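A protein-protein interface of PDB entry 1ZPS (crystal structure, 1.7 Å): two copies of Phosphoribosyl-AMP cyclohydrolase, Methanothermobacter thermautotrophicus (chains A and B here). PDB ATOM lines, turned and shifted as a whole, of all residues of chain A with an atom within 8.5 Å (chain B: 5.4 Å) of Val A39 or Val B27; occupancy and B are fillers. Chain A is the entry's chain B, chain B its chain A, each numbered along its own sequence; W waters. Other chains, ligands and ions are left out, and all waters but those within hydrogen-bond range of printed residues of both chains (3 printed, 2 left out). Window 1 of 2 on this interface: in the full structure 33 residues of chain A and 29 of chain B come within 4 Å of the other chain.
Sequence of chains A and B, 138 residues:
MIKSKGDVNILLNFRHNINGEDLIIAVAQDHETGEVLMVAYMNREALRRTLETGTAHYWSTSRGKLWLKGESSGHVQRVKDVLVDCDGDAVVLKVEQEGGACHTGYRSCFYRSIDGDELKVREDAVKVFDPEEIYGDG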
ATOM      1  N   ILE A  24       6.907 -37.232  -2.189  1.00  0.00           N
ATOM      2  CA  ILE A  24       5.931 -37.113  -1.117  1.00  0.00           C
ATOM      3  C   ILE A  24       5.208 -35.813  -1.456  1.00  0.00           C
ATOM      4  O   ILE A  24       5.748 -34.963  -2.171  1.00  0.00           O
ATOM      5  CB  ILE A  24       6.556 -36.975   0.303  1.00  0.00           C
ATOM      6  CG1 ILE A  24       7.603 -35.863   0.325  1.00  0.00           C
ATOM      7  CG2 ILE A  24       7.108 -38.313   0.758  1.00  0.00           C
ATOM      8  CD1 ILE A  24       8.064 -35.508   1.727  1.00  0.00           C
ATOM      9  N   ILE A  25       3.979 -35.678  -0.974  1.00  0.00           N
ATOM     10  CA  ILE A  25       3.186 -34.479  -1.215  1.00  0.00           C
ATOM     11  C   ILE A  25       3.482 -33.494  -0.088  1.00  0.00           C
ATOM     12  O   ILE A  25       3.510 -33.878   1.079  1.00  0.00           O
ATOM     13  CB  ILE A  25       1.684 -34.817  -1.221  1.00  0.00           C
ATOM     14  CG1 ILE A  25       1.373 -35.737  -2.406  1.00  0.00           C
ATOM     15  CG2 ILE A  25       0.859 -33.537  -1.289  1.00  0.00           C
ATOM     16  CD1 ILE A  25      -0.022 -36.337  -2.375  1.00  0.00           C
ATOM     17  N   ALA A  26       3.706 -32.233  -0.441  1.00  0.00           N
ATOM     18  CA  ALA A  26       4.007 -31.204   0.551  1.00  0.00           C
ATOM     19  C   ALA A  26       3.005 -30.054   0.488  1.00  0.00           C
ATOM     20  O   ALA A  26       2.722 -29.516  -0.582  1.00  0.00           O
ATOM     21  CB  ALA A  26       5.416 -30.670   0.330  1.00  0.00           C
ATOM     22  N   VAL A  27       2.470 -29.688   1.647  1.00  0.00           N
ATOM     23  CA  VAL A  27       1.517 -28.591   1.737  1.00  0.00           C
ATOM     24  C   VAL A  27       2.164 -27.471   2.545  1.00  0.00           C
ATOM     25  O   VAL A  27       2.565 -27.690   3.682  1.00  0.00           O
ATOM     26  CB  VAL A  27       0.224 -29.030   2.461  1.00  0.00           C
ATOM     27  CG1 VAL A  27      -0.784 -27.886   2.468  1.00  0.00           C
ATOM     28  CG2 VAL A  27      -0.363 -30.255   1.785  1.00  0.00           C
ATOM     29  N   ALA A  28       2.281 -26.286   1.951  1.00  0.00           N
ATOM     30  CA  ALA A  28       2.859 -25.135   2.644  1.00  0.00           C
ATOM     31  C   ALA A  28       1.718 -24.353   3.289  1.00  0.00           C
ATOM     32  O   ALA A  28       0.759 -23.984   2.614  1.00  0.00           O
ATOM     33  CB  ALA A  28       3.615 -24.248   1.662  1.00  0.00           C
ATOM     34  N   GLN A  29       1.835 -24.096   4.588  1.00  0.00           N
ATOM     35  CA  GLN A  29       0.800 -23.386   5.337  1.00  0.00           C
ATOM     36  C   GLN A  29       1.381 -22.261   6.194  1.00  0.00           C
ATOM     37  O   GLN A  29       2.407 -22.437   6.843  1.00  0.00           O
ATOM     38  CB  GLN A  29       0.048 -24.391   6.223  1.00  0.00           C
ATOM     39  CG  GLN A  29      -0.933 -23.789   7.226  1.00  0.00           C
ATOM     40  CD  GLN A  29      -1.663 -24.852   8.022  1.00  0.00           C
ATOM     41  OE1 GLN A  29      -1.051 -25.790   8.536  1.00  0.00           O
ATOM     42  NE2 GLN A  29      -2.981 -24.707   8.139  1.00  0.00           N
ATOM     43  N   GLY A  34      -2.668 -19.946   9.321  1.00  0.00           N
ATOM     44  CA  GLY A  34      -3.181 -21.261   8.975  1.00  0.00           C
ATOM     45  C   GLY A  34      -3.620 -21.403   7.527  1.00  0.00           C
ATOM     46  O   GLY A  34      -4.061 -22.476   7.110  1.00  0.00           O
ATOM     47  N   VAL A  36      -3.561 -22.139   3.705  1.00  0.00           N
ATOM     48  CA  VAL A  36      -2.768 -23.018   2.852  1.00  0.00           C
ATOM     49  C   VAL A  36      -2.264 -22.157   1.698  1.00  0.00           C
ATOM     50  O   VAL A  36      -3.054 -21.592   0.936  1.00  0.00           O
ATOM     51  CB  VAL A  36      -3.609 -24.196   2.318  1.00  0.00           C
ATOM     52  CG1 VAL A  36      -2.814 -24.991   1.288  1.00  0.00           C
ATOM     53  CG2 VAL A  36      -4.017 -25.103   3.472  1.00  0.00           C
ATOM     54  N   LEU A  37      -0.942 -22.058   1.586  1.00  0.00           N
ATOM     55  CA  LEU A  37      -0.306 -21.237   0.565  1.00  0.00           C
ATOM     56  C   LEU A  37      -0.054 -21.933  -0.764  1.00  0.00           C
ATOM     57  O   LEU A  37      -0.145 -21.305  -1.821  1.00  0.00           O
ATOM     58  CB  LEU A  37       1.011 -20.678   1.111  1.00  0.00           C
ATOM     59  CG  LEU A  37       0.896 -19.856   2.401  1.00  0.00           C
ATOM     60  CD1 LEU A  37       2.260 -19.351   2.819  1.00  0.00           C
ATOM     61  CD2 LEU A  37      -0.060 -18.686   2.178  1.00  0.00           C
ATOM     62  N   MET A  38       0.273 -23.221  -0.723  1.00  0.00           N
ATOM     63  CA  MET A  38       0.535 -23.953  -1.956  1.00  0.00           C
ATOM     64  C   MET A  38       0.720 -25.438  -1.706  1.00  0.00           C
ATOM     65  O   MET A  38       0.957 -25.866  -0.576  1.00  0.00           O
ATOM     66  CB  MET A  38       1.795 -23.406  -2.640  1.00  0.00           C
ATOM     67  CG  MET A  38       3.061 -23.548  -1.805  1.00  0.00           C
ATOM     68  SD  MET A  38       4.566 -23.067  -2.688  1.00  0.00           S
ATOM     69  CE  MET A  38       4.991 -24.601  -3.490  1.00  0.00           C
ATOM     70  N   VAL A  39       0.592 -26.215  -2.776  1.00  0.00           N
ATOM     71  CA  VAL A  39       0.781 -27.660  -2.724  1.00  0.00           C
ATOM     72  C   VAL A  39       1.814 -27.999  -3.790  1.00  0.00           C
ATOM     73  O   VAL A  39       1.744 -27.493  -4.911  1.00  0.00           O
ATOM     74  CB  VAL A  39      -0.528 -28.420  -3.043  1.00  0.00           C
ATOM     75  CG1 VAL A  39      -0.229 -29.890  -3.309  1.00  0.00           C
ATOM     76  CG2 VAL A  39      -1.503 -28.280  -1.883  1.00  0.00           C
ATOM     77  N   ALA A  40       2.774 -28.846  -3.435  1.00  0.00           N
ATOM     78  CA  ALA A  40       3.816 -29.253  -4.371  1.00  0.00           C
ATOM     79  C   ALA A  40       4.396 -30.586  -3.922  1.00  0.00           C
ATOM     80  O   ALA A  40       4.009 -31.125  -2.890  1.00  0.00           O
ATOM     81  CB  ALA A  40       4.916 -28.197  -4.430  1.00  0.00           C
ATOM     82  N   TYR A  41       5.319 -31.121  -4.708  1.00  0.00           N
ATOM     83  CA  TYR A  41       5.955 -32.386  -4.370  1.00  0.00           C
ATOM     84  C   TYR A  41       7.375 -32.146  -3.883  1.00  0.00           C
ATOM     85  O   TYR A  41       7.943 -31.076  -4.091  1.00  0.00           O
ATOM     86  CB  TYR A  41       6.028 -33.294  -5.601  1.00  0.00           C
ATOM     87  CG  TYR A  41       4.704 -33.873  -6.044  1.00  0.00           C
ATOM     88  CD1 TYR A  41       4.127 -34.941  -5.364  1.00  0.00           C
ATOM     89  CD2 TYR A  41       4.037 -33.358  -7.154  1.00  0.00           C
ATOM     90  CE1 TYR A  41       2.910 -35.491  -5.783  1.00  0.00           C
ATOM     91  CE2 TYR A  41       2.823 -33.895  -7.580  1.00  0.00           C
ATOM     92  CZ  TYR A  41       2.268 -34.961  -6.890  1.00  0.00           C
ATOM     93  OH  TYR A  41       1.078 -35.507  -7.318  1.00  0.00           O
ATOM     94  N   MET A  42       7.935 -33.157  -3.228  1.00  0.00           N
ATOM     95  CA  MET A  42       9.314 -33.118  -2.756  1.00  0.00           C
ATOM     96  C   MET A  42       9.890 -34.497  -3.006  1.00  0.00           C
ATOM     97  O   MET A  42       9.219 -35.504  -2.769  1.00  0.00           O
ATOM     98  CB  MET A  42       9.414 -32.869  -1.249  1.00  0.00           C
ATOM     99  CG  MET A  42       9.044 -31.496  -0.753  1.00  0.00           C
ATOM    100  SD  MET A  42       9.346 -31.463   1.034  1.00  0.00           S
ATOM    101  CE  MET A  42       9.610 -29.710   1.304  1.00  0.00           C
ATOM    102  N   TYR A  58      11.434 -27.748  -3.149  1.00  0.00           N
ATOM    103  CA  TYR A  58      10.456 -28.639  -3.758  1.00  0.00           C
ATOM    104  C   TYR A  58      11.028 -29.289  -5.007  1.00  0.00           C
ATOM    105  O   TYR A  58      12.120 -28.943  -5.454  1.00  0.00           O
ATOM    106  CB  TYR A  58       9.203 -27.854  -4.142  1.00  0.00           C
ATOM    107  CG  TYR A  58       8.520 -27.173  -2.985  1.00  0.00           C
ATOM    108  CD1 TYR A  58       7.785 -27.906  -2.059  1.00  0.00           C
ATOM    109  CD2 TYR A  58       8.607 -25.790  -2.815  1.00  0.00           C
ATOM    110  CE1 TYR A  58       7.149 -27.285  -0.991  1.00  0.00           C
ATOM    111  CE2 TYR A  58       7.975 -25.156  -1.746  1.00  0.00           C
ATOM    112  CZ  TYR A  58       7.250 -25.910  -0.840  1.00  0.00           C
ATOM    113  OH  TYR A  58       6.634 -25.300   0.228  1.00  0.00           O
ATOM    114  N   TRP A  59      10.282 -30.238  -5.560  1.00  0.00           N
ATOM    115  CA  TRP A  59      10.689 -30.908  -6.785  1.00  0.00           C
ATOM    116  C   TRP A  59       9.712 -30.498  -7.868  1.00  0.00           C
ATOM    117  O   TRP A  59       8.506 -30.697  -7.733  1.00  0.00           O
ATOM    118  CB  TRP A  59      10.665 -32.428  -6.613  1.00  0.00           C
ATOM    119  CG  TRP A  59      10.749 -33.176  -7.915  1.00  0.00           C
ATOM    120  CD1 TRP A  59       9.704 -33.616  -8.675  1.00  0.00           C
ATOM    121  CD2 TRP A  59      11.939 -33.541  -8.620  1.00  0.00           C
ATOM    122  NE1 TRP A  59      10.169 -34.236  -9.808  1.00  0.00           N
ATOM    123  CE2 TRP A  59      11.538 -34.205  -9.802  1.00  0.00           C
ATOM    124  CE3 TRP A  59      13.307 -33.373  -8.369  1.00  0.00           C
ATOM    125  CZ2 TRP A  59      12.456 -34.703 -10.732  1.00  0.00           C
ATOM    126  CZ3 TRP A  59      14.222 -33.869  -9.296  1.00  0.00           C
ATOM    127  CH2 TRP A  59      13.789 -34.526 -10.462  1.00  0.00           C
ATOM    128  N   TRP A  67      13.999 -27.310  -6.608  1.00  0.00           N
ATOM    129  CA  TRP A  67      14.275 -25.888  -6.601  1.00  0.00           C
ATOM    130  C   TRP A  67      13.917 -25.267  -5.261  1.00  0.00           C
ATOM    131  O   TRP A  67      13.015 -25.732  -4.561  1.00  0.00           O
ATOM    132  CB  TRP A  67      13.516 -25.196  -7.743  1.00  0.00           C
ATOM    133  CG  TRP A  67      12.212 -24.549  -7.367  1.00  0.00           C
ATOM    134  CD1 TRP A  67      12.015 -23.242  -7.025  1.00  0.00           C
ATOM    135  CD2 TRP A  67      10.925 -25.172  -7.324  1.00  0.00           C
ATOM    136  NE1 TRP A  67      10.686 -23.010  -6.776  1.00  0.00           N
ATOM    137  CE2 TRP A  67       9.993 -24.178  -6.952  1.00  0.00           C
ATOM    138  CE3 TRP A  67      10.467 -26.474  -7.565  1.00  0.00           C
ATOM    139  CZ2 TRP A  67       8.628 -24.445  -6.814  1.00  0.00           C
ATOM    140  CZ3 TRP A  67       9.107 -26.738  -7.428  1.00  0.00           C
ATOM    141  CH2 TRP A  67       8.205 -25.726  -7.056  1.00  0.00           C
ATOM    142  N   GLN A  77      10.460 -19.411   1.854  1.00  0.00           N
ATOM    143  CA  GLN A  77       9.560 -19.872   2.900  1.00  0.00           C
ATOM    144  C   GLN A  77      10.405 -20.445   4.026  1.00  0.00           C
ATOM    145  O   GLN A  77      11.034 -21.488   3.869  1.00  0.00           O
ATOM    146  CB  GLN A  77       8.616 -20.954   2.364  1.00  0.00           C
ATOM    147  CG  GLN A  77       7.804 -20.529   1.152  1.00  0.00           C
ATOM    148  CD  GLN A  77       6.931 -21.646   0.640  1.00  0.00           C
ATOM    149  OE1 GLN A  77       7.317 -22.815   0.687  1.00  0.00           O
ATOM    150  NE2 GLN A  77       5.752 -21.295   0.131  1.00  0.00           N
ATOM    151  N   VAL A  91       3.677 -34.206   3.883  1.00  0.00           N
ATOM    152  CA  VAL A  91       4.022 -33.330   4.994  1.00  0.00           C
ATOM    153  C   VAL A  91       3.334 -31.981   4.860  1.00  0.00           C
ATOM    154  O   VAL A  91       2.915 -31.585   3.773  1.00  0.00           O
ATOM    155  CB  VAL A  91       5.552 -33.053   5.064  1.00  0.00           C
ATOM    156  CG1 VAL A  91       6.311 -34.338   5.342  1.00  0.00           C
ATOM    157  CG2 VAL A  91       6.033 -32.418   3.758  1.00  0.00           C
ATOM    158  N   VAL A  92       3.208 -31.293   5.986  1.00  0.00           N
ATOM    159  CA  VAL A  92       2.648 -29.950   6.015  1.00  0.00           C
ATOM    160  C   VAL A  92       3.791 -29.111   6.560  1.00  0.00           C
ATOM    161  O   VAL A  92       4.345 -29.425   7.611  1.00  0.00           O
ATOM    162  CB  VAL A  92       1.451 -29.828   6.977  1.00  0.00           C
ATOM    163  CG1 VAL A  92       1.088 -28.355   7.167  1.00  0.00           C
ATOM    164  CG2 VAL A  92       0.264 -30.592   6.427  1.00  0.00           C
ATOM    165  N   ALA A 101       3.416 -16.571  -2.192  1.00  0.00           N
ATOM    166  CA  ALA A 101       3.750 -17.931  -2.584  1.00  0.00           C
ATOM    167  C   ALA A 101       3.481 -18.188  -4.064  1.00  0.00           C
ATOM    168  O   ALA A 101       4.068 -19.091  -4.661  1.00  0.00           O
ATOM    169  CB  ALA A 101       2.957 -18.920  -1.736  1.00  0.00           C
ATOM    170  N   SER A 108      -1.315 -16.572  -1.662  1.00  0.00           N
ATOM    171  CA  SER A 108      -1.593 -17.998  -1.768  1.00  0.00           C
ATOM    172  C   SER A 108      -1.962 -18.384  -3.196  1.00  0.00           C
ATOM    173  O   SER A 108      -2.572 -17.601  -3.924  1.00  0.00           O
ATOM    174  CB  SER A 108      -2.742 -18.378  -0.828  1.00  0.00           C
ATOM    175  OG  SER A 108      -3.164 -19.711  -1.057  1.00  0.00           O
ATOM    176  N   CYS A 109      -1.584 -19.593  -3.597  1.00  0.00           N
ATOM    177  CA  CYS A 109      -1.911 -20.084  -4.929  1.00  0.00           C
ATOM    178  C   CYS A 109      -3.414 -20.276  -5.024  1.00  0.00           C
ATOM    179  O   CYS A 109      -3.989 -20.220  -6.109  1.00  0.00           O
ATOM    180  CB  CYS A 109      -1.240 -21.430  -5.197  1.00  0.00           C
ATOM    181  SG  CYS A 109       0.500 -21.334  -5.585  1.00  0.00           S
ATOM    182  N   PHE A 110      -4.038 -20.516  -3.877  1.00  0.00           N
ATOM    183  CA  PHE A 110      -5.475 -20.745  -3.816  1.00  0.00           C
ATOM    184  C   PHE A 110      -6.242 -19.439  -3.655  1.00  0.00           C
ATOM    185  O   PHE A 110      -6.916 -19.216  -2.649  1.00  0.00           O
ATOM    186  CB  PHE A 110      -5.799 -21.705  -2.666  1.00  0.00           C
ATOM    187  CG  PHE A 110      -5.135 -23.049  -2.799  1.00  0.00           C
ATOM    188  CD1 PHE A 110      -3.838 -23.256  -2.332  1.00  0.00           C
ATOM    189  CD2 PHE A 110      -5.791 -24.098  -3.433  1.00  0.00           C
ATOM    190  CE1 PHE A 110      -3.203 -24.493  -2.499  1.00  0.00           C
ATOM    191  CE2 PHE A 110      -5.171 -25.334  -3.606  1.00  0.00           C
ATOM    192  CZ  PHE A 110      -3.874 -25.534  -3.140  1.00  0.00           C
ATOM    193  N   ILE B  25      -4.895 -32.959  -6.488  1.00  0.00           N
ATOM    194  CA  ILE B  25      -4.609 -33.157  -5.074  1.00  0.00           C
ATOM    195  C   ILE B  25      -5.600 -32.346  -4.249  1.00  0.00           C
ATOM    196  O   ILE B  25      -5.839 -31.171  -4.527  1.00  0.00           O
ATOM    197  CB  ILE B  25      -3.166 -32.719  -4.732  1.00  0.00           C
ATOM    198  CG1 ILE B  25      -2.174 -33.617  -5.478  1.00  0.00           C
ATOM    199  CG2 ILE B  25      -2.937 -32.783  -3.229  1.00  0.00           C
ATOM    200  CD1 ILE B  25      -0.724 -33.241  -5.280  1.00  0.00           C
ATOM    201  N   ALA B  26      -6.188 -32.985  -3.246  1.00  0.00           N
ATOM    202  CA  ALA B  26      -7.154 -32.323  -2.384  1.00  0.00           C
ATOM    203  C   ALA B  26      -6.645 -32.232  -0.950  1.00  0.00           C
ATOM    204  O   ALA B  26      -6.190 -33.223  -0.375  1.00  0.00           O
ATOM    205  CB  ALA B  26      -8.492 -33.072  -2.424  1.00  0.00           C
ATOM    206  N   VAL B  27      -6.709 -31.031  -0.385  1.00  0.00           N
ATOM    207  CA  VAL B  27      -6.274 -30.804   0.983  1.00  0.00           C
ATOM    208  C   VAL B  27      -7.514 -30.497   1.813  1.00  0.00           C
ATOM    209  O   VAL B  27      -8.184 -29.486   1.588  1.00  0.00           O
ATOM    210  CB  VAL B  27      -5.307 -29.598   1.085  1.00  0.00           C
ATOM    211  CG1 VAL B  27      -4.840 -29.418   2.527  1.00  0.00           C
ATOM    212  CG2 VAL B  27      -4.124 -29.799   0.160  1.00  0.00           C
ATOM    213  N   ALA B  28      -7.832 -31.383   2.750  1.00  0.00           N
ATOM    214  CA  ALA B  28      -8.986 -31.181   3.617  1.00  0.00           C
ATOM    215  C   ALA B  28      -8.537 -30.341   4.801  1.00  0.00           C
ATOM    216  O   ALA B  28      -7.662 -30.746   5.568  1.00  0.00           O
ATOM    217  CB  ALA B  28      -9.535 -32.520   4.097  1.00  0.00           C
ATOM    218  N   GLN B  29      -9.136 -29.163   4.943  1.00  0.00           N
ATOM    219  CA  GLN B  29      -8.786 -28.252   6.024  1.00  0.00           C
ATOM    220  C   GLN B  29     -10.012 -27.886   6.854  1.00  0.00           C
ATOM    221  O   GLN B  29     -11.069 -27.573   6.304  1.00  0.00           O
ATOM    222  CB  GLN B  29      -8.150 -26.981   5.444  1.00  0.00           C
ATOM    223  CG  GLN B  29      -7.846 -25.899   6.471  1.00  0.00           C
ATOM    224  CD  GLN B  29      -7.226 -24.661   5.850  1.00  0.00           C
ATOM    225  OE1 GLN B  29      -7.644 -24.214   4.782  1.00  0.00           O
ATOM    226  NE2 GLN B  29      -6.236 -24.091   6.523  1.00  0.00           N
ATOM    227  N   VAL B  36      -4.938 -28.552   8.884  1.00  0.00           N
ATOM    228  CA  VAL B  36      -4.969 -29.452   7.742  1.00  0.00           C
ATOM    229  C   VAL B  36      -5.253 -30.836   8.320  1.00  0.00           C
ATOM    230  O   VAL B  36      -4.500 -31.337   9.155  1.00  0.00           O
ATOM    231  CB  VAL B  36      -3.616 -29.445   6.987  1.00  0.00           C
ATOM    232  CG1 VAL B  36      -3.641 -30.460   5.849  1.00  0.00           C
ATOM    233  CG2 VAL B  36      -3.347 -28.048   6.436  1.00  0.00           C
ATOM    234  N   MET B  38      -6.021 -33.792   6.326  1.00  0.00           N
ATOM    235  CA  MET B  38      -5.496 -34.872   5.496  1.00  0.00           C
ATOM    236  C   MET B  38      -5.320 -34.401   4.061  1.00  0.00           C
ATOM    237  O   MET B  38      -5.808 -33.339   3.677  1.00  0.00           O
ATOM    238  CB  MET B  38      -6.470 -36.054   5.487  1.00  0.00           C
ATOM    239  CG  MET B  38      -7.844 -35.692   4.918  1.00  0.00           C
ATOM    240  SD  MET B  38      -8.981 -37.085   4.717  1.00  0.00           S
ATOM    241  CE  MET B  38      -8.519 -37.657   3.099  1.00  0.00           C
ATOM    242  N   VAL B  39      -4.612 -35.206   3.276  1.00  0.00           N
ATOM    243  CA  VAL B  39      -4.412 -34.923   1.864  1.00  0.00           C
ATOM    244  C   VAL B  39      -4.726 -36.216   1.122  1.00  0.00           C
ATOM    245  O   VAL B  39      -4.427 -37.307   1.607  1.00  0.00           O
ATOM    246  CB  VAL B  39      -2.958 -34.475   1.542  1.00  0.00           C
ATOM    247  CG1 VAL B  39      -2.673 -33.137   2.197  1.00  0.00           C
ATOM    248  CG2 VAL B  39      -1.963 -35.526   2.005  1.00  0.00           C
ATOM    249  N   ALA B  40      -5.355 -36.092  -0.040  1.00  0.00           N
ATOM    250  CA  ALA B  40      -5.711 -37.255  -0.843  1.00  0.00           C
ATOM    251  C   ALA B  40      -6.007 -36.806  -2.264  1.00  0.00           C
ATOM    252  O   ALA B  40      -6.204 -35.620  -2.519  1.00  0.00           O
ATOM    253  CB  ALA B  40      -6.930 -37.956  -0.251  1.00  0.00           C
ATOM    254  N   ASP B  85      -6.231 -24.166  -7.012  1.00  0.00           N
ATOM    255  CA  ASP B  85      -4.838 -23.805  -7.285  1.00  0.00           C
ATOM    256  C   ASP B  85      -4.760 -22.947  -8.549  1.00  0.00           C
ATOM    257  O   ASP B  85      -5.653 -22.998  -9.396  1.00  0.00           O
ATOM    258  CB  ASP B  85      -4.013 -25.088  -7.475  1.00  0.00           C
ATOM    259  CG  ASP B  85      -2.515 -24.853  -7.383  1.00  0.00           C
ATOM    260  OD1 ASP B  85      -2.086 -23.684  -7.251  1.00  0.00           O
ATOM    261  OD2 ASP B  85      -1.762 -25.849  -7.448  1.00  0.00           O
ATOM    262  N   ALA B  90      -5.003 -28.650  -8.041  1.00  0.00           N
ATOM    263  CA  ALA B  90      -5.045 -28.878  -6.606  1.00  0.00           C
ATOM    264  C   ALA B  90      -6.180 -28.056  -6.009  1.00  0.00           C
ATOM    265  O   ALA B  90      -6.485 -26.964  -6.484  1.00  0.00           O
ATOM    266  CB  ALA B  90      -3.712 -28.490  -5.962  1.00  0.00           C
ATOM    267  N   VAL B  91      -6.817 -28.589  -4.976  1.00  0.00           N
ATOM    268  CA  VAL B  91      -7.906 -27.876  -4.332  1.00  0.00           C
ATOM    269  C   VAL B  91      -7.813 -27.975  -2.821  1.00  0.00           C
ATOM    270  O   VAL B  91      -7.214 -28.906  -2.281  1.00  0.00           O
ATOM    271  CB  VAL B  91      -9.291 -28.436  -4.759  1.00  0.00           C
ATOM    272  CG1 VAL B  91      -9.478 -28.288  -6.264  1.00  0.00           C
ATOM    273  CG2 VAL B  91      -9.413 -29.899  -4.346  1.00  0.00           C
ATOM    274  N   VAL B  92      -8.397 -26.997  -2.145  1.00  0.00           N
ATOM    275  CA  VAL B  92      -8.438 -26.993  -0.698  1.00  0.00           C
ATOM    276  C   VAL B  92      -9.902 -27.124  -0.318  1.00  0.00           C
ATOM    277  O   VAL B  92     -10.730 -26.310  -0.729  1.00  0.00           O
ATOM    278  CB  VAL B  92      -7.885 -25.685  -0.104  1.00  0.00           C
ATOM    279  CG1 VAL B  92      -8.207 -25.619   1.386  1.00  0.00           C
ATOM    280  CG2 VAL B  92      -6.379 -25.620  -0.315  1.00  0.00           C
ATOM    281  N   LEU B  93     -10.223 -28.165   0.440  1.00  0.00           N
ATOM    282  CA  LEU B  93     -11.596 -28.376   0.871  1.00  0.00           C
ATOM    283  C   LEU B  93     -11.766 -27.871   2.296  1.00  0.00           C
ATOM    284  O   LEU B  93     -11.153 -28.395   3.226  1.00  0.00           O
ATOM    285  CB  LEU B  93     -11.961 -29.863   0.824  1.00  0.00           C
ATOM    286  CG  LEU B  93     -11.762 -30.643  -0.475  1.00  0.00           C
ATOM    287  CD1 LEU B  93     -12.212 -32.080  -0.258  1.00  0.00           C
ATOM    288  CD2 LEU B  93     -12.546 -30.001  -1.602  1.00  0.00           C
ATOM    289  N   LYS B  94     -12.580 -26.831   2.452  1.00  0.00           N
ATOM    290  CA  LYS B  94     -12.877 -26.269   3.764  1.00  0.00           C
ATOM    291  C   LYS B  94     -13.982 -27.183   4.269  1.00  0.00           C
ATOM    292  O   LYS B  94     -15.071 -27.208   3.696  1.00  0.00           O
ATOM    293  CB  LYS B  94     -13.407 -24.844   3.620  1.00  0.00           C
ATOM    294  CG  LYS B  94     -12.387 -23.844   3.109  1.00  0.00           C
ATOM    295  CD  LYS B  94     -11.401 -23.466   4.196  1.00  0.00           C
ATOM    296  CE  LYS B  94     -10.550 -22.279   3.774  1.00  0.00           C
ATOM    297  NZ  LYS B  94      -9.756 -21.742   4.911  1.00  0.00           N
HETATM  298  O   HOH W   1      -2.288 -27.720   9.972  1.00  0.00           O
HETATM  299  O   HOH W   2      -6.515 -22.117   3.647  1.00  0.00           O
HETATM  300  O   HOH W   3      -6.227 -19.952  -8.128  1.00  0.00           O
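Printed residues of chain B within 4 Å of Val A27: Val B39 (3.7 Å).
Of the printed residues of chain B, Gln A29 touches Gln B29 (3.7 Å) and Val B36 (3.8 Å).
Val A39 touches just these residues of chain B: Ile B25 (3.9 Å) and Val B27 (3.7 Å).
No residue of chain A comes within 4 Å of Ala B26.
Of chain A, only Val A39 (3.7 Å) comes within 4 Å of Val B27.
Printed residues of chain A within 4 Å of Asp B85: Cys A109 and Phe A110.
Of the printed residues of chain A, Val B91 touches Phe A110 (3.8 Å).
Of the printed residues of chain A, Val B92 touches Val A36 (3.96 Å) and Phe A110 (3.5 Å).
The backbone carbonyl oxygen of Val B27 lies within hydrogen-bond range of the backbone NH of Leu B93 (2.7 Å).
The backbone NH (N) of Gln B29 is in hydrogen-bond range of the backbone carbonyl oxygen (O) of Leu B93, at 2.8 Å.
NZ of Lys B94 sits at hydrogen-bond distance from OE1 of Gln B29 (3.3 Å).
The side-chain amide nitrogen (NE2) of Gln A29 lies within hydrogen-bond range of the backbone carbonyl oxygen (O) of Gly A34.
O of Val A36 lies within hydrogen-bond range of OG of Ser A108 (2.7 Å).
The backbone carbonyl oxygen (O) of Tyr A41 lies within hydrogen-bond range of the backbone NH (N) of Trp A59 (2.9 Å).
The side-chain amide nitrogen (NE2) of Gln B29 sits at hydrogen-bond distance from the backbone carbonyl oxygen (O) of Gly A34 (2.8 Å).
Of the 15 printed residues of chain B, 9 touch a printed residue of chain A.
Hydrophobic or aromatic side chains of chain A within 4 Å of the printed part of chain B: Val A27, Val A36, Val A39, Tyr A41, Val A92 and Phe A110.
Among the printed residues, 15 pairs touch across the chains.
Water W2 lies within hydrogen-bond range of OE1 of Gln B29 (2.6 Å), N of Val A36 (3.0 Å) and NZ of Lys B94 (3.5 Å).
Water W1 lies within hydrogen-bond range of OE1 of Gln A29 (2.7 Å) and N of Val B36 (3.0 Å).
Water W3 lies within hydrogen-bond range of the backbone carbonyl oxygen of Cys A109 (3.0 Å) and the backbone carbonyl oxygen of Asp B85 (3.3 Å).
CG2 of Val A27 touches CG1 of Val B39, at 3.7 Å.
Gln A29 touches Gln B29.
Gln A29 touches Val B36.
Gln B29 touches Val A36 (NE2 to CG2, 3.9 Å).
Val B92 touches Val A36 (CG2 to CG1, 3.96 Å).
Ile B25 touches Val A39 (CD1 to CG1, 3.9 Å).
Tyr A41 touches Ile B25.
N of Asp B85 touches CD2 of Phe A110, 3.6 Å away.
O of Ala B90 touches CE2 of Phe A110, at 3.6 Å.
Val B91 touches Phe A110.
Val A27 touches Val B39, and with the chains exchanged Val A39 touches Val B27.
Gln A29 touches its own counterpart, Gln B29.
Val A36 touches Val B92, and with the chains exchanged Val A92 touches Val B36.
Val A39 touches Ile B25, but with the chains exchanged Ile A25 does not touch Val B39 (4.8 Å).
Positions printed for both chains: 25, 26, 27, 28, 29, 36, 38, 39, 40, 91 and 92.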
